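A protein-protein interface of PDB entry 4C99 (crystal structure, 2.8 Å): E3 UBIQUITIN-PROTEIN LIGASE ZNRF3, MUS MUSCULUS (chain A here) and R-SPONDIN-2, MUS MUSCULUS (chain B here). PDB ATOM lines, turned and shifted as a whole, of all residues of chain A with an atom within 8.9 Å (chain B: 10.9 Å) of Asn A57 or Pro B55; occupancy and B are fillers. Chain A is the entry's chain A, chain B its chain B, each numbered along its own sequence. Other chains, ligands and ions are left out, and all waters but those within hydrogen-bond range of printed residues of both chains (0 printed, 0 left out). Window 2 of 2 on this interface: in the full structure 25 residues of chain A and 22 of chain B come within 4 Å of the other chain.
ND2 of Asn A57 is in hydrogen-bond range of OD2 of Asp B56, 3.1 Å away.
The side-chain sulfur (SG) of Cys A55 forms a disulfide with the side-chain sulfur (SG) of Cys A84 (2.1 Å). The side-chain sulfur (SG) of Cys A84 lies within hydrogen-bond range of the side-chain amino group (NZ) of Lys A90, at 3.8 Å. The backbone carbonyl oxygen (O) of His B52 sits at hydrogen-bond distance from the backbone NH (N) of Arg B59 (3.0 Å). The side-chain carboxylate of Asp B56 is in salt-bridge range of the guanidinium group of Arg B59 (2.6 Å).
Arg B21 touches Leu A52. Leu A52 touches Arg B59. Asp B56 touches Cys A55 (OD2 to SG, 3.98 Å). Asn A57 touches Pro B55. Cys A84 touches Asp B56.
Of the printed residues of chain B, Leu A52 touches Arg B21 (3.5 Å) and Arg B59 (3.6 Å). Of the printed residues of chain B, Cys A55 touches Asp B56. No residue of chain B comes within 4 Å of Asn A56. Asn A57 touches just these residues of chain B: Pro B55 (3.6 Å) and Asp B56 (3.1 Å). No residue of chain B comes within 4 Å of Asn A58. Cys A84 touches just one residue of chain B: Asp B56 (3.8 Å). Printed residues of chain A within 4 Å of Arg B21: Leu A52. Ala B54 touches none of the printed residues of chain A. Pro B55 touches one residue of chain A. Printed residues of chain A within 4 Å of Asp B56: Cys A55, Asn A57 and Cys A84. Printed residues of chain A within 4 Å of Arg B59: Leu A52. The nearest residue of chain A that does not touch Pro B55 is Asn A58 (6.5 Å). The nearest printed residue of chain A that does not touch Arg B59 is Cys A55 (4.3 Å).
Printed residues of chain B that touch a printed residue of chain A: Arg B21, Pro B55, Asp B56 and Arg B59. Of the 16 printed residues of chain A, 4 touch a printed residue of chain B. Hydrophobic or aromatic side chains of chain A that line the printed part of chain B: Leu A52. Among the printed residues, 6 pairs touch across the chains. Among the printed residues, no Asp or Glu carboxylate lies within 4 Å of a Lys or Arg side-chain nitrogen of the other chain.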
ATOM      1  N   LEU A  52      34.904 -25.979  19.431  1.00  0.00           N
ATOM      2  CA  LEU A  52      33.514 -25.796  19.887  1.00  0.00           C
ATOM      3  C   LEU A  52      33.471 -25.649  21.388  1.00  0.00           C
ATOM      4  O   LEU A  52      32.465 -25.984  22.022  1.00  0.00           O
ATOM      5  CB  LEU A  52      32.612 -26.994  19.511  1.00  0.00           C
ATOM      6  CG  LEU A  52      32.910 -27.690  18.188  1.00  0.00           C
ATOM      7  CD1 LEU A  52      31.993 -28.895  18.049  1.00  0.00           C
ATOM      8  CD2 LEU A  52      32.851 -26.742  16.993  1.00  0.00           C
ATOM      9  N   GLY A  53      34.578 -25.235  21.972  1.00  0.00           N
ATOM     10  CA  GLY A  53      34.615 -24.917  23.383  1.00  0.00           C
ATOM     11  C   GLY A  53      35.017 -23.472  23.541  1.00  0.00           C
ATOM     12  O   GLY A  53      35.309 -22.994  24.642  1.00  0.00           O
ATOM     13  N   LEU A  54      35.063 -22.753  22.440  1.00  0.00           N
ATOM     14  CA  LEU A  54      35.437 -21.366  22.548  1.00  0.00           C
ATOM     15  C   LEU A  54      34.428 -20.520  21.810  1.00  0.00           C
ATOM     16  O   LEU A  54      34.669 -19.987  20.733  1.00  0.00           O
ATOM     17  CB  LEU A  54      36.857 -21.174  22.074  1.00  0.00           C
ATOM     18  CG  LEU A  54      37.837 -21.849  23.029  1.00  0.00           C
ATOM     19  CD1 LEU A  54      39.211 -21.830  22.411  1.00  0.00           C
ATOM     20  CD2 LEU A  54      37.858 -21.145  24.368  1.00  0.00           C
ATOM     21  N   CYS A  55      33.258 -20.467  22.426  1.00  0.00           N
ATOM     22  CA  CYS A  55      32.197 -19.591  22.046  1.00  0.00           C
ATOM     23  C   CYS A  55      31.879 -18.755  23.272  1.00  0.00           C
ATOM     24  O   CYS A  55      31.903 -19.271  24.397  1.00  0.00           O
ATOM     25  CB  CYS A  55      31.003 -20.435  21.658  1.00  0.00           C
ATOM     26  SG  CYS A  55      31.394 -21.628  20.370  1.00  0.00           S
ATOM     27  N   ASN A  56      31.604 -17.467  23.069  1.00  0.00           N
ATOM     28  CA  ASN A  56      31.114 -16.629  24.157  1.00  0.00           C
ATOM     29  C   ASN A  56      29.652 -16.950  24.455  1.00  0.00           C
ATOM     30  O   ASN A  56      29.141 -16.613  25.525  1.00  0.00           O
ATOM     31  CB  ASN A  56      31.284 -15.142  23.842  1.00  0.00           C
ATOM     32  CG  ASN A  56      31.211 -14.274  25.091  1.00  0.00           C
ATOM     33  OD1 ASN A  56      31.192 -14.785  26.219  1.00  0.00           O
ATOM     34  ND2 ASN A  56      31.159 -12.959  24.896  1.00  0.00           N
ATOM     35  N   ASN A  57      29.008 -17.623  23.496  1.00  0.00           N
ATOM     36  CA  ASN A  57      27.591 -18.012  23.556  1.00  0.00           C
ATOM     37  C   ASN A  57      27.072 -18.435  24.935  1.00  0.00           C
ATOM     38  O   ASN A  57      26.178 -17.785  25.486  1.00  0.00           O
ATOM     39  CB  ASN A  57      27.297 -19.146  22.545  1.00  0.00           C
ATOM     40  CG  ASN A  57      27.277 -18.672  21.090  1.00  0.00           C
ATOM     41  OD1 ASN A  57      27.073 -17.492  20.800  1.00  0.00           O
ATOM     42  ND2 ASN A  57      27.477 -19.606  20.169  1.00  0.00           N
ATOM     43  N   ASN A  58      27.622 -19.514  25.488  1.00  0.00           N
ATOM     44  CA  ASN A  58      27.020 -20.138  26.673  1.00  0.00           C
ATOM     45  C   ASN A  58      26.962 -19.190  27.872  1.00  0.00           C
ATOM     46  O   ASN A  58      27.823 -18.314  28.021  1.00  0.00           O
ATOM     47  CB  ASN A  58      27.743 -21.439  27.058  1.00  0.00           C
ATOM     48  CG  ASN A  58      26.896 -22.340  27.948  1.00  0.00           C
ATOM     49  OD1 ASN A  58      25.668 -22.366  27.842  1.00  0.00           O
ATOM     50  ND2 ASN A  58      27.552 -23.087  28.825  1.00  0.00           N
ATOM     51  N   ASP A  59      25.930 -19.370  28.701  1.00  0.00           N
ATOM     52  CA  ASP A  59      25.717 -18.567  29.909  1.00  0.00           C
ATOM     53  C   ASP A  59      27.021 -18.500  30.729  1.00  0.00           C
ATOM     54  O   ASP A  59      27.423 -17.420  31.168  1.00  0.00           O
ATOM     55  CB  ASP A  59      24.556 -19.158  30.738  1.00  0.00           C
ATOM     56  CG  ASP A  59      23.837 -18.124  31.622  1.00  0.00           C
ATOM     57  OD1 ASP A  59      23.911 -16.896  31.369  1.00  0.00           O
ATOM     58  OD2 ASP A  59      23.154 -18.565  32.576  1.00  0.00           O
ATOM     59  N   GLU A  60      27.676 -19.652  30.906  1.00  0.00           N
ATOM     60  CA  GLU A  60      29.024 -19.728  31.493  1.00  0.00           C
ATOM     61  C   GLU A  60      29.648 -21.113  31.339  1.00  0.00           C
ATOM     62  O   GLU A  60      28.963 -22.097  31.053  1.00  0.00           O
ATOM     63  CB  GLU A  60      29.019 -19.349  32.978  1.00  0.00           C
ATOM     64  CG  GLU A  60      29.496 -17.935  33.288  1.00  0.00           C
ATOM     65  CD  GLU A  60      30.423 -17.902  34.493  1.00  0.00           C
ATOM     66  OE1 GLU A  60      31.633 -18.161  34.328  1.00  0.00           O
ATOM     67  OE2 GLU A  60      29.942 -17.625  35.609  1.00  0.00           O
ATOM     68  N   GLU A  61      30.957 -21.167  31.571  1.00  0.00           N
ATOM     69  CA  GLU A  61      31.760 -22.363  31.374  1.00  0.00           C
ATOM     70  C   GLU A  61      32.513 -22.756  32.659  1.00  0.00           C
ATOM     71  O   GLU A  61      32.262 -22.218  33.741  1.00  0.00           O
ATOM     72  CB  GLU A  61      32.736 -22.122  30.216  1.00  0.00           C
ATOM     73  CG  GLU A  61      32.070 -21.699  28.913  1.00  0.00           C
ATOM     74  CD  GLU A  61      31.939 -20.191  28.745  1.00  0.00           C
ATOM     75  OE1 GLU A  61      31.704 -19.466  29.742  1.00  0.00           O
ATOM     76  OE2 GLU A  61      32.068 -19.726  27.592  1.00  0.00           O
ATOM     77  N   LYS A  82      29.838 -23.433  10.031  1.00  0.00           N
ATOM     78  CA  LYS A  82      29.486 -22.109  10.535  1.00  0.00           C
ATOM     79  C   LYS A  82      29.958 -22.072  11.978  1.00  0.00           C
ATOM     80  O   LYS A  82      29.365 -22.720  12.847  1.00  0.00           O
ATOM     81  CB  LYS A  82      27.977 -21.878  10.497  1.00  0.00           C
ATOM     82  CG  LYS A  82      27.378 -21.740   9.113  1.00  0.00           C
ATOM     83  CD  LYS A  82      25.896 -21.392   9.238  1.00  0.00           C
ATOM     84  CE  LYS A  82      25.130 -21.497   7.921  1.00  0.00           C
ATOM     85  NZ  LYS A  82      23.659 -21.475   8.164  1.00  0.00           N
ATOM     86  N   PRO A  83      31.048 -21.348  12.235  1.00  0.00           N
ATOM     87  CA  PRO A  83      31.626 -21.294  13.577  1.00  0.00           C
ATOM     88  C   PRO A  83      31.105 -20.132  14.407  1.00  0.00           C
ATOM     89  O   PRO A  83      30.810 -19.077  13.857  1.00  0.00           O
ATOM     90  CB  PRO A  83      33.116 -21.131  13.298  1.00  0.00           C
ATOM     91  CG  PRO A  83      33.189 -20.463  11.965  1.00  0.00           C
ATOM     92  CD  PRO A  83      31.917 -20.731  11.223  1.00  0.00           C
ATOM     93  N   CYS A  84      31.011 -20.326  15.721  1.00  0.00           N
ATOM     94  CA  CYS A  84      30.457 -19.300  16.617  1.00  0.00           C
ATOM     95  C   CYS A  84      31.175 -17.940  16.480  1.00  0.00           C
ATOM     96  O   CYS A  84      30.508 -16.914  16.346  1.00  0.00           O
ATOM     97  CB  CYS A  84      30.404 -19.780  18.088  1.00  0.00           C
ATOM     98  SG  CYS A  84      31.944 -20.446  18.781  1.00  0.00           S
ATOM     99  N   LEU A  85      32.516 -17.941  16.470  1.00  0.00           N
ATOM    100  CA  LEU A  85      33.322 -16.700  16.294  1.00  0.00           C
ATOM    101  C   LEU A  85      34.491 -16.991  15.362  1.00  0.00           C
ATOM    102  O   LEU A  85      34.692 -18.148  14.967  1.00  0.00           O
ATOM    103  CB  LEU A  85      33.878 -16.172  17.626  1.00  0.00           C
ATOM    104  CG  LEU A  85      33.186 -16.618  18.918  1.00  0.00           C
ATOM    105  CD1 LEU A  85      34.171 -16.709  20.061  1.00  0.00           C
ATOM    106  CD2 LEU A  85      32.033 -15.717  19.296  1.00  0.00           C
ATOM    107  N   LYS A  90      38.073 -16.758  18.864  1.00  0.00           N
ATOM    108  CA  LYS A  90      38.317 -17.822  19.847  1.00  0.00           C
ATOM    109  C   LYS A  90      39.653 -17.623  20.585  1.00  0.00           C
ATOM    110  O   LYS A  90      39.840 -18.157  21.663  1.00  0.00           O
ATOM    111  CB  LYS A  90      38.323 -19.171  19.183  1.00  0.00           C
ATOM    112  CG  LYS A  90      37.081 -19.488  18.359  1.00  0.00           C
ATOM    113  CD  LYS A  90      37.293 -20.813  17.640  1.00  0.00           C
ATOM    114  CE  LYS A  90      36.158 -21.787  17.859  1.00  0.00           C
ATOM    115  NZ  LYS A  90      35.046 -21.569  16.899  1.00  0.00           N
ATOM    116  N   ARG A  93      38.781 -15.162  23.324  1.00  0.00           N
ATOM    117  CA  ARG A  93      38.030 -15.864  24.369  1.00  0.00           C
ATOM    118  C   ARG A  93      38.867 -16.710  25.317  1.00  0.00           C
ATOM    119  O   ARG A  93      38.400 -17.118  26.367  1.00  0.00           O
ATOM    120  CB  ARG A  93      36.940 -16.763  23.761  1.00  0.00           C
ATOM    121  CG  ARG A  93      35.569 -16.123  23.645  1.00  0.00           C
ATOM    122  CD  ARG A  93      35.027 -15.714  25.013  1.00  0.00           C
ATOM    123  NE  ARG A  93      34.416 -16.808  25.781  1.00  0.00           N
ATOM    124  CZ  ARG A  93      34.304 -16.816  27.111  1.00  0.00           C
ATOM    125  NH1 ARG A  93      34.814 -15.817  27.848  1.00  0.00           N
ATOM    126  NH2 ARG A  93      33.706 -17.840  27.715  1.00  0.00           N
ATOM    127  N   ARG B  21      30.802 -31.735  16.411  1.00  0.00           N
ATOM    128  CA  ARG B  21      29.458 -31.488  15.875  1.00  0.00           C
ATOM    129  C   ARG B  21      28.574 -32.731  15.957  1.00  0.00           C
ATOM    130  O   ARG B  21      28.138 -33.289  14.949  1.00  0.00           O
ATOM    131  CB  ARG B  21      29.540 -30.947  14.448  1.00  0.00           C
ATOM    132  CG  ARG B  21      28.186 -30.557  13.870  1.00  0.00           C
ATOM    133  CD  ARG B  21      28.272 -29.396  12.888  1.00  0.00           C
ATOM    134  NE  ARG B  21      27.576 -29.745  11.649  1.00  0.00           N
ATOM    135  CZ  ARG B  21      28.162 -30.105  10.504  1.00  0.00           C
ATOM    136  NH1 ARG B  21      29.486 -30.146  10.385  1.00  0.00           N
ATOM    137  NH2 ARG B  21      27.410 -30.419   9.455  1.00  0.00           N
ATOM    138  N   GLN B  24      22.637 -34.438  15.604  1.00  0.00           N
ATOM    139  CA  GLN B  24      21.693 -33.582  16.333  1.00  0.00           C
ATOM    140  C   GLN B  24      20.854 -34.299  17.382  1.00  0.00           C
ATOM    141  O   GLN B  24      20.632 -33.734  18.443  1.00  0.00           O
ATOM    142  CB  GLN B  24      20.782 -32.811  15.368  1.00  0.00           C
ATOM    143  CG  GLN B  24      21.519 -31.744  14.572  1.00  0.00           C
ATOM    144  CD  GLN B  24      20.652 -30.538  14.277  1.00  0.00           C
ATOM    145  OE1 GLN B  24      19.770 -30.581  13.422  1.00  0.00           O
ATOM    146  NE2 GLN B  24      20.907 -29.449  14.986  1.00  0.00           N
ATOM    147  N   TYR B  50      22.591 -30.729  31.414  1.00  0.00           N
ATOM    148  CA  TYR B  50      21.268 -30.951  30.846  1.00  0.00           C
ATOM    149  C   TYR B  50      21.211 -30.616  29.359  1.00  0.00           C
ATOM    150  O   TYR B  50      21.864 -29.671  28.894  1.00  0.00           O
ATOM    151  CB  TYR B  50      20.231 -30.125  31.622  1.00  0.00           C
ATOM    152  CG  TYR B  50      20.286 -28.678  31.253  1.00  0.00           C
ATOM    153  CD1 TYR B  50      21.211 -27.834  31.823  1.00  0.00           C
ATOM    154  CD2 TYR B  50      19.453 -28.179  30.291  1.00  0.00           C
ATOM    155  CE1 TYR B  50      21.293 -26.508  31.451  1.00  0.00           C
ATOM    156  CE2 TYR B  50      19.528 -26.864  29.904  1.00  0.00           C
ATOM    157  CZ  TYR B  50      20.444 -26.035  30.483  1.00  0.00           C
ATOM    158  OH  TYR B  50      20.484 -24.737  30.081  1.00  0.00           O
ATOM    159  N   GLY B  51      20.411 -31.387  28.623  1.00  0.00           N
ATOM    160  CA  GLY B  51      20.172 -31.104  27.217  1.00  0.00           C
ATOM    161  C   GLY B  51      19.773 -29.657  27.022  1.00  0.00           C
ATOM    162  O   GLY B  51      19.076 -29.089  27.838  1.00  0.00           O
ATOM    163  N   HIS B  52      20.204 -29.049  25.940  1.00  0.00           N
ATOM    164  CA  HIS B  52      19.942 -27.635  25.753  1.00  0.00           C
ATOM    165  C   HIS B  52      20.282 -27.358  24.329  1.00  0.00           C
ATOM    166  O   HIS B  52      21.233 -27.910  23.801  1.00  0.00           O
ATOM    167  CB  HIS B  52      20.788 -26.789  26.720  1.00  0.00           C
ATOM    168  CG  HIS B  52      20.879 -25.336  26.365  1.00  0.00           C
ATOM    169  ND1 HIS B  52      22.038 -24.606  26.530  1.00  0.00           N
ATOM    170  CD2 HIS B  52      19.970 -24.475  25.856  1.00  0.00           C
ATOM    171  CE1 HIS B  52      21.841 -23.359  26.141  1.00  0.00           C
ATOM    172  NE2 HIS B  52      20.595 -23.254  25.720  1.00  0.00           N
ATOM    173  N   ARG B  53      19.472 -26.531  23.694  1.00  0.00           N
ATOM    174  CA  ARG B  53      19.664 -26.210  22.306  1.00  0.00           C
ATOM    175  C   ARG B  53      20.323 -24.854  22.283  1.00  0.00           C
ATOM    176  O   ARG B  53      19.678 -23.834  22.506  1.00  0.00           O
ATOM    177  CB  ARG B  53      18.317 -26.244  21.557  1.00  0.00           C
ATOM    178  CG  ARG B  53      17.519 -27.533  21.815  1.00  0.00           C
ATOM    179  CD  ARG B  53      16.373 -27.762  20.833  1.00  0.00           C
ATOM    180  NE  ARG B  53      16.857 -28.090  19.488  1.00  0.00           N
ATOM    181  CZ  ARG B  53      16.095 -28.245  18.402  1.00  0.00           C
ATOM    182  NH1 ARG B  53      14.766 -28.112  18.465  1.00  0.00           N
ATOM    183  NH2 ARG B  53      16.674 -28.531  17.236  1.00  0.00           N
ATOM    184  N   ALA B  54      21.632 -24.861  22.054  1.00  0.00           N
ATOM    185  CA  ALA B  54      22.388 -23.637  21.813  1.00  0.00           C
ATOM    186  C   ALA B  54      22.157 -23.154  20.374  1.00  0.00           C
ATOM    187  O   ALA B  54      21.638 -23.911  19.540  1.00  0.00           O
ATOM    188  CB  ALA B  54      23.868 -23.881  22.067  1.00  0.00           C
ATOM    189  N   PRO B  55      22.534 -21.892  20.076  1.00  0.00           N
ATOM    190  CA  PRO B  55      22.355 -21.413  18.702  1.00  0.00           C
ATOM    191  C   PRO B  55      22.948 -22.395  17.692  1.00  0.00           C
ATOM    192  O   PRO B  55      22.216 -22.942  16.856  1.00  0.00           O
ATOM    193  CB  PRO B  55      23.113 -20.068  18.679  1.00  0.00           C
ATOM    194  CG  PRO B  55      23.900 -20.011  19.953  1.00  0.00           C
ATOM    195  CD  PRO B  55      23.161 -20.868  20.935  1.00  0.00           C
ATOM    196  N   ASP B  56      24.256 -22.642  17.819  1.00  0.00           N
ATOM    197  CA  ASP B  56      24.990 -23.554  16.927  1.00  0.00           C
ATOM    198  C   ASP B  56      24.620 -25.046  17.075  1.00  0.00           C
ATOM    199  O   ASP B  56      24.559 -25.756  16.080  1.00  0.00           O
ATOM    200  CB  ASP B  56      26.523 -23.340  17.047  1.00  0.00           C
ATOM    201  CG  ASP B  56      27.030 -23.297  18.504  1.00  0.00           C
ATOM    202  OD1 ASP B  56      26.688 -24.196  19.294  1.00  0.00           O
ATOM    203  OD2 ASP B  56      27.787 -22.365  18.855  1.00  0.00           O
ATOM    204  N   MET B  57      24.356 -25.513  18.293  1.00  0.00           N
ATOM    205  CA  MET B  57      24.052 -26.930  18.513  1.00  0.00           C
ATOM    206  C   MET B  57      23.454 -27.283  19.888  1.00  0.00           C
ATOM    207  O   MET B  57      23.388 -26.467  20.799  1.00  0.00           O
ATOM    208  CB  MET B  57      25.329 -27.750  18.335  1.00  0.00           C
ATOM    209  CG  MET B  57      26.344 -27.552  19.449  1.00  0.00           C
ATOM    210  SD  MET B  57      27.970 -28.138  18.966  1.00  0.00           S
ATOM    211  CE  MET B  57      28.341 -26.964  17.651  1.00  0.00           C
ATOM    212  N   ASN B  58      23.073 -28.543  20.027  1.00  0.00           N
ATOM    213  CA  ASN B  58      22.471 -29.038  21.249  1.00  0.00           C
ATOM    214  C   ASN B  58      23.490 -29.743  22.171  1.00  0.00           C
ATOM    215  O   ASN B  58      23.873 -30.915  21.961  1.00  0.00           O
ATOM    216  CB  ASN B  58      21.297 -29.951  20.894  1.00  0.00           C
ATOM    217  CG  ASN B  58      20.458 -29.394  19.751  1.00  0.00           C
ATOM    218  OD1 ASN B  58      20.359 -28.174  19.553  1.00  0.00           O
ATOM    219  ND2 ASN B  58      19.868 -30.289  18.979  1.00  0.00           N
ATOM    220  N   ARG B  59      23.914 -29.006  23.199  1.00  0.00           N
ATOM    221  CA  ARG B  59      25.033 -29.414  24.043  1.00  0.00           C
ATOM    222  C   ARG B  59      24.654 -29.462  25.505  1.00  0.00           C
ATOM    223  O   ARG B  59      24.038 -28.531  26.012  1.00  0.00           O
ATOM    224  CB  ARG B  59      26.219 -28.457  23.870  1.00  0.00           C
ATOM    225  CG  ARG B  59      25.878 -26.974  23.817  1.00  0.00           C
ATOM    226  CD  ARG B  59      27.056 -26.098  24.259  1.00  0.00           C
ATOM    227  NE  ARG B  59      28.135 -25.933  23.265  1.00  0.00           N
ATOM    228  CZ  ARG B  59      28.046 -25.196  22.150  1.00  0.00           C
ATOM    229  NH1 ARG B  59      26.912 -24.571  21.849  1.00  0.00           N
ATOM    230  NH2 ARG B  59      29.086 -25.087  21.323  1.00  0.00           N
ATOM    231  N   CYS B  60      25.032 -30.548  26.178  1.00  0.00           N
ATOM    232  CA  CYS B  60      25.000 -30.596  27.620  1.00  0.00           C
ATOM    233  C   CYS B  60      25.557 -29.302  28.227  1.00  0.00           C
ATOM    234  O   CYS B  60      26.518 -28.740  27.713  1.00  0.00           O
ATOM    235  CB  CYS B  60      25.840 -31.759  28.124  1.00  0.00           C
ATOM    236  SG  CYS B  60      25.276 -33.392  27.607  1.00  0.00           S
ATOM    237  N   ALA B  61      24.939 -28.816  29.306  1.00  0.00           N
ATOM    238  CA  ALA B  61      25.420 -27.610  29.998  1.00  0.00           C
ATOM    239  C   ALA B  61      25.273 -27.779  31.483  1.00  0.00           C
ATOM    240  O   ALA B  61      24.543 -28.654  31.950  1.00  0.00           O
ATOM    241  CB  ALA B  61      24.703 -26.348  29.513  1.00  0.00           C
ATOM    242  N   LYS B  74      18.498 -23.930  33.103  1.00  0.00           N
ATOM    243  CA  LYS B  74      19.744 -23.489  33.745  1.00  0.00           C
ATOM    244  C   LYS B  74      19.573 -23.396  35.266  1.00  0.00           C
ATOM    245  O   LYS B  74      20.476 -23.794  36.016  1.00  0.00           O
ATOM    246  CB  LYS B  74      20.230 -22.141  33.179  1.00  0.00           C
